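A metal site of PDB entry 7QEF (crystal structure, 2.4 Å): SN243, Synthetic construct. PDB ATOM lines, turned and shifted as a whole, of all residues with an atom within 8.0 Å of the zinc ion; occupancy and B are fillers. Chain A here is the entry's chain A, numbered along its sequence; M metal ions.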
ATOM      1  N   GLU A  20     -19.919  22.689 -19.593  1.00  0.00           N
ATOM      2  CA  GLU A  20     -18.513  22.854 -20.053  1.00  0.00           C
ATOM      3  C   GLU A  20     -18.368  22.529 -21.536  1.00  0.00           C
ATOM      4  O   GLU A  20     -19.330  22.036 -22.143  1.00  0.00           O
ATOM      5  CB  GLU A  20     -17.571  21.994 -19.206  1.00  0.00           C
ATOM      6  CG  GLU A  20     -17.149  22.673 -17.923  1.00  0.00           C
ATOM      7  CD  GLU A  20     -16.494  24.034 -18.129  1.00  0.00           C
ATOM      8  OE1 GLU A  20     -15.937  24.259 -19.225  1.00  0.00           O
ATOM      9  OE2 GLU A  20     -16.546  24.868 -17.211  1.00  0.00           O
ATOM     10  N   ILE A  22     -16.569  20.518 -24.761  1.00  0.00           N
ATOM     11  CA  ILE A  22     -15.933  19.198 -25.035  1.00  0.00           C
ATOM     12  C   ILE A  22     -15.289  19.255 -26.424  1.00  0.00           C
ATOM     13  O   ILE A  22     -15.945  19.761 -27.360  1.00  0.00           O
ATOM     14  CB  ILE A  22     -16.976  18.071 -24.924  1.00  0.00           C
ATOM     15  CG1 ILE A  22     -18.037  18.170 -26.027  1.00  0.00           C
ATOM     16  CG2 ILE A  22     -17.599  18.054 -23.542  1.00  0.00           C
ATOM     17  CD1 ILE A  22     -19.081  17.088 -25.957  1.00  0.00           C
ATOM     18  N   ARG A  30     -20.301  22.457 -26.999  1.00  0.00           N
ATOM     19  CA  ARG A  30     -20.851  22.671 -25.631  1.00  0.00           C
ATOM     20  C   ARG A  30     -21.615  21.421 -25.197  1.00  0.00           C
ATOM     21  O   ARG A  30     -22.569  21.038 -25.907  1.00  0.00           O
ATOM     22  CB  ARG A  30     -21.760  23.901 -25.600  1.00  0.00           C
ATOM     23  CG  ARG A  30     -21.054  25.213 -25.907  1.00  0.00           C
ATOM     24  CD  ARG A  30     -21.723  26.366 -25.182  1.00  0.00           C
ATOM     25  NE  ARG A  30     -23.132  26.512 -25.527  1.00  0.00           N
ATOM     26  CZ  ARG A  30     -24.003  27.207 -24.822  1.00  0.00           C
ATOM     27  NH1 ARG A  30     -25.264  27.281 -25.210  1.00  0.00           N
ATOM     28  NH2 ARG A  30     -23.624  27.818 -23.708  1.00  0.00           N
ATOM     29  N   ASP A  31     -21.224  20.828 -24.075  1.00  0.00           N
ATOM     30  CA  ASP A  31     -21.951  19.657 -23.554  1.00  0.00           C
ATOM     31  C   ASP A  31     -23.086  20.143 -22.673  1.00  0.00           C
ATOM     32  O   ASP A  31     -22.939  20.316 -21.463  1.00  0.00           O
ATOM     33  CB  ASP A  31     -21.027  18.719 -22.784  1.00  0.00           C
ATOM     34  CG  ASP A  31     -21.680  17.364 -22.520  1.00  0.00           C
ATOM     35  OD1 ASP A  31     -22.615  17.019 -23.258  1.00  0.00           O
ATOM     36  OD2 ASP A  31     -21.278  16.662 -21.574  1.00  0.00           O
ATOM     37  N   LEU A  32     -24.254  20.287 -23.288  1.00  0.00           N
ATOM     38  CA  LEU A  32     -25.373  20.942 -22.629  1.00  0.00           C
ATOM     39  C   LEU A  32     -26.216  20.002 -21.792  1.00  0.00           C
ATOM     40  O   LEU A  32     -26.804  20.450 -20.788  1.00  0.00           O
ATOM     41  CB  LEU A  32     -26.239  21.653 -23.678  1.00  0.00           C
ATOM     42  CG  LEU A  32     -25.475  22.810 -24.342  1.00  0.00           C
ATOM     43  CD1 LEU A  32     -26.118  23.258 -25.655  1.00  0.00           C
ATOM     44  CD2 LEU A  32     -25.311  24.013 -23.394  1.00  0.00           C
ATOM     45  N   ASN A  33     -26.290  18.707 -22.162  1.00  0.00           N
ATOM     46  CA  ASN A  33     -26.913  17.704 -21.295  1.00  0.00           C
ATOM     47  C   ASN A  33     -25.995  17.283 -20.169  1.00  0.00           C
ATOM     48  O   ASN A  33     -26.458  16.579 -19.262  1.00  0.00           O
ATOM     49  CB  ASN A  33     -27.351  16.453 -22.056  1.00  0.00           C
ATOM     50  CG  ASN A  33     -26.287  15.923 -22.970  1.00  0.00           C
ATOM     51  OD1 ASN A  33     -25.094  16.048 -22.680  1.00  0.00           O
ATOM     52  ND2 ASN A  33     -26.707  15.273 -24.052  1.00  0.00           N
ATOM     53  N   ASP A  34     -24.711  17.658 -20.210  1.00  0.00           N
ATOM     54  CA  ASP A  34     -23.753  17.341 -19.158  1.00  0.00           C
ATOM     55  C   ASP A  34     -23.668  15.836 -18.947  1.00  0.00           C
ATOM     56  O   ASP A  34     -23.620  15.336 -17.824  1.00  0.00           O
ATOM     57  CB  ASP A  34     -24.116  18.105 -17.870  1.00  0.00           C
ATOM     58  CG  ASP A  34     -23.160  17.858 -16.716  1.00  0.00           C
ATOM     59  OD1 ASP A  34     -21.997  18.346 -16.713  1.00  0.00           O
ATOM     60  OD2 ASP A  34     -23.615  17.168 -15.779  1.00  0.00           O
ATOM     61  N   ASN A  35     -23.635  15.121 -20.083  1.00  0.00           N
ATOM     62  CA  ASN A  35     -23.516  13.647 -20.078  1.00  0.00           C
ATOM     63  C   ASN A  35     -22.057  13.281 -20.332  1.00  0.00           C
ATOM     64  O   ASN A  35     -21.680  12.126 -20.102  1.00  0.00           O
ATOM     65  CB  ASN A  35     -24.367  13.016 -21.178  1.00  0.00           C
ATOM     66  CG  ASN A  35     -23.947  13.440 -22.567  1.00  0.00           C
ATOM     67  OD1 ASN A  35     -23.069  14.287 -22.729  1.00  0.00           O
ATOM     68  ND2 ASN A  35     -24.571  12.863 -23.583  1.00  0.00           N
ATOM     69  N   GLY A  36     -21.265  14.246 -20.813  1.00  0.00           N
ATOM     70  CA  GLY A  36     -19.839  14.019 -21.072  1.00  0.00           C
ATOM     71  C   GLY A  36     -19.606  13.600 -22.507  1.00  0.00           C
ATOM     72  O   GLY A  36     -18.448  13.309 -22.859  1.00  0.00           O
ATOM     73  N   GLU A  37     -20.664  13.558 -23.307  1.00  0.00           N
ATOM     74  CA  GLU A  37     -20.516  13.071 -24.701  1.00  0.00           C
ATOM     75  C   GLU A  37     -21.188  14.057 -25.657  1.00  0.00           C
ATOM     76  O   GLU A  37     -22.079  14.805 -25.222  1.00  0.00           O
ATOM     77  CB  GLU A  37     -21.109  11.668 -24.834  1.00  0.00           C
ATOM     78  CG  GLU A  37     -20.533  10.891 -25.998  1.00  0.00           C
ATOM     79  CD  GLU A  37     -20.770   9.393 -25.948  1.00  0.00           C
ATOM     80  OE1 GLU A  37     -21.649   8.968 -25.181  1.00  0.00           O
ATOM     81  OE2 GLU A  37     -20.068   8.663 -26.670  1.00  0.00           O
ATOM     82  N   LEU A  38     -20.753  14.051 -26.923  1.00  0.00           N
ATOM     83  CA  LEU A  38     -21.330  14.986 -27.913  1.00  0.00           C
ATOM     84  C   LEU A  38     -22.637  14.403 -28.436  1.00  0.00           C
ATOM     85  O   LEU A  38     -22.602  13.319 -29.037  1.00  0.00           O
ATOM     86  CB  LEU A  38     -20.334  15.174 -29.068  1.00  0.00           C
ATOM     87  CG  LEU A  38     -20.856  16.011 -30.240  1.00  0.00           C
ATOM     88  CD1 LEU A  38     -21.250  17.405 -29.786  1.00  0.00           C
ATOM     89  CD2 LEU A  38     -19.821  16.084 -31.347  1.00  0.00           C
ATOM     90  N   ASP A  39     -23.749  15.113 -28.224  1.00  0.00           N
ATOM     91  CA  ASP A  39     -25.036  14.656 -28.799  1.00  0.00           C
ATOM     92  C   ASP A  39     -25.245  15.406 -30.109  1.00  0.00           C
ATOM     93  O   ASP A  39     -24.774  16.552 -30.215  1.00  0.00           O
ATOM     94  CB  ASP A  39     -26.170  14.803 -27.783  1.00  0.00           C
ATOM     95  CG  ASP A  39     -25.864  14.179 -26.444  1.00  0.00           C
ATOM     96  OD1 ASP A  39     -24.830  14.542 -25.846  1.00  0.00           O
ATOM     97  OD2 ASP A  39     -26.653  13.331 -26.003  1.00  0.00           O
ATOM     98  N   PRO A  40     -25.897  14.798 -31.126  1.00  0.00           N
ATOM     99  CA  PRO A  40     -26.040  15.451 -32.421  1.00  0.00           C
ATOM    100  C   PRO A  40     -26.603  16.876 -32.316  1.00  0.00           C
ATOM    101  O   PRO A  40     -26.293  17.683 -33.170  1.00  0.00           O
ATOM    102  CB  PRO A  40     -27.040  14.533 -33.147  1.00  0.00           C
ATOM    103  CG  PRO A  40     -26.797  13.172 -32.526  1.00  0.00           C
ATOM    104  CD  PRO A  40     -26.478  13.463 -31.082  1.00  0.00           C
ATOM    105  N   TYR A  41     -27.418  17.161 -31.299  1.00  0.00           N
ATOM    106  CA  TYR A  41     -28.030  18.499 -31.153  1.00  0.00           C
ATOM    107  C   TYR A  41     -26.962  19.494 -30.674  1.00  0.00           C
ATOM    108  O   TYR A  41     -27.082  20.685 -31.007  1.00  0.00           O
ATOM    109  CB  TYR A  41     -29.259  18.443 -30.232  1.00  0.00           C
ATOM    110  CG  TYR A  41     -29.022  18.675 -28.763  1.00  0.00           C
ATOM    111  CD1 TYR A  41     -28.956  19.954 -28.240  1.00  0.00           C
ATOM    112  CD2 TYR A  41     -28.911  17.610 -27.871  1.00  0.00           C
ATOM    113  CE1 TYR A  41     -28.760  20.174 -26.887  1.00  0.00           C
ATOM    114  CE2 TYR A  41     -28.715  17.819 -26.517  1.00  0.00           C
ATOM    115  CZ  TYR A  41     -28.644  19.106 -26.023  1.00  0.00           C
ATOM    116  OH  TYR A  41     -28.444  19.314 -24.683  1.00  0.00           O
ATOM    117  N   GLU A  42     -25.962  19.006 -29.945  1.00  0.00           N
ATOM    118  CA  GLU A  42     -24.852  19.871 -29.467  1.00  0.00           C
ATOM    119  C   GLU A  42     -23.800  20.006 -30.569  1.00  0.00           C
ATOM    120  O   GLU A  42     -22.851  20.778 -30.383  1.00  0.00           O
ATOM    121  CB  GLU A  42     -24.267  19.266 -28.195  1.00  0.00           C
ATOM    122  CG  GLU A  42     -25.278  19.032 -27.096  1.00  0.00           C
ATOM    123  CD  GLU A  42     -24.784  18.194 -25.930  1.00  0.00           C
ATOM    124  OE1 GLU A  42     -23.846  17.410 -26.128  1.00  0.00           O
ATOM    125  OE2 GLU A  42     -25.349  18.331 -24.834  1.00  0.00           O
ATOM    126  N   ASP A  54     -32.749  15.407 -32.607  1.00  0.00           N
ATOM    127  CA  ASP A  54     -32.058  14.812 -31.467  1.00  0.00           C
ATOM    128  C   ASP A  54     -32.435  15.497 -30.159  1.00  0.00           C
ATOM    129  O   ASP A  54     -32.539  14.845 -29.111  1.00  0.00           O
ATOM    130  CB  ASP A  54     -30.541  14.856 -31.661  1.00  0.00           C
ATOM    131  CG  ASP A  54     -29.794  14.094 -30.588  1.00  0.00           C
ATOM    132  OD1 ASP A  54     -29.852  12.844 -30.611  1.00  0.00           O
ATOM    133  OD2 ASP A  54     -29.173  14.738 -29.710  1.00  0.00           O
ATOM    134  N   GLN A  58     -34.910  13.784 -26.929  1.00  0.00           N
ATOM    135  CA  GLN A  58     -34.512  13.650 -25.537  1.00  0.00           C
ATOM    136  C   GLN A  58     -35.376  14.402 -24.553  1.00  0.00           C
ATOM    137  O   GLN A  58     -35.088  14.367 -23.353  1.00  0.00           O
ATOM    138  CB  GLN A  58     -33.078  14.162 -25.343  1.00  0.00           C
ATOM    139  CG  GLN A  58     -32.032  13.565 -26.225  1.00  0.00           C
ATOM    140  CD  GLN A  58     -30.701  14.244 -26.054  1.00  0.00           C
ATOM    141  OE1 GLN A  58     -30.357  14.673 -24.944  1.00  0.00           O
ATOM    142  NE2 GLN A  58     -29.942  14.345 -27.126  1.00  0.00           N
HETATM  143 ZN    ZN M   1     -23.802  15.920 -24.346  1.00  0.00          ZN
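The side-chain carboxylate (OD1) of Asp 31 is bound to the zinc ion (1.9 Å). The zinc ion is bound by the side-chain amide oxygen (OD1) of Asn 33, 2.1 Å away. The backbone carbonyl oxygen (O) of Glu 37 is bound to the zinc ion, 2.2 Å away. OD1 of Asp 39 binds the zinc ion. The side-chain carboxylate (OE1) of Glu 42 is bound to the zinc ion (2.3 Å). OD1 of Asn 35 binds the zinc ion.
Within 4 Å of the zinc ion: Asp 31, Asn 33, Asn 35, Glu 37, Asp 39 and Glu 42.
N of Asn 33 lies within hydrogen-bond range of OH of Tyr 41 (3.4 Å). N of Asp 31 lies within hydrogen-bond range of O of Glu 20 (3.0 Å). The side-chain carboxylate (OD2) of Asp 31 sits at hydrogen-bond distance from the backbone NH (N) of Gly 36. The side-chain carboxylate (OE2) of Glu 42 lies within hydrogen-bond range of the backbone NH (N) of Leu 32 (2.7 Å). The side-chain carboxylate of Glu 42 lies within hydrogen-bond range of the side-chain hydroxyl of Tyr 41, at 3.3 Å.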
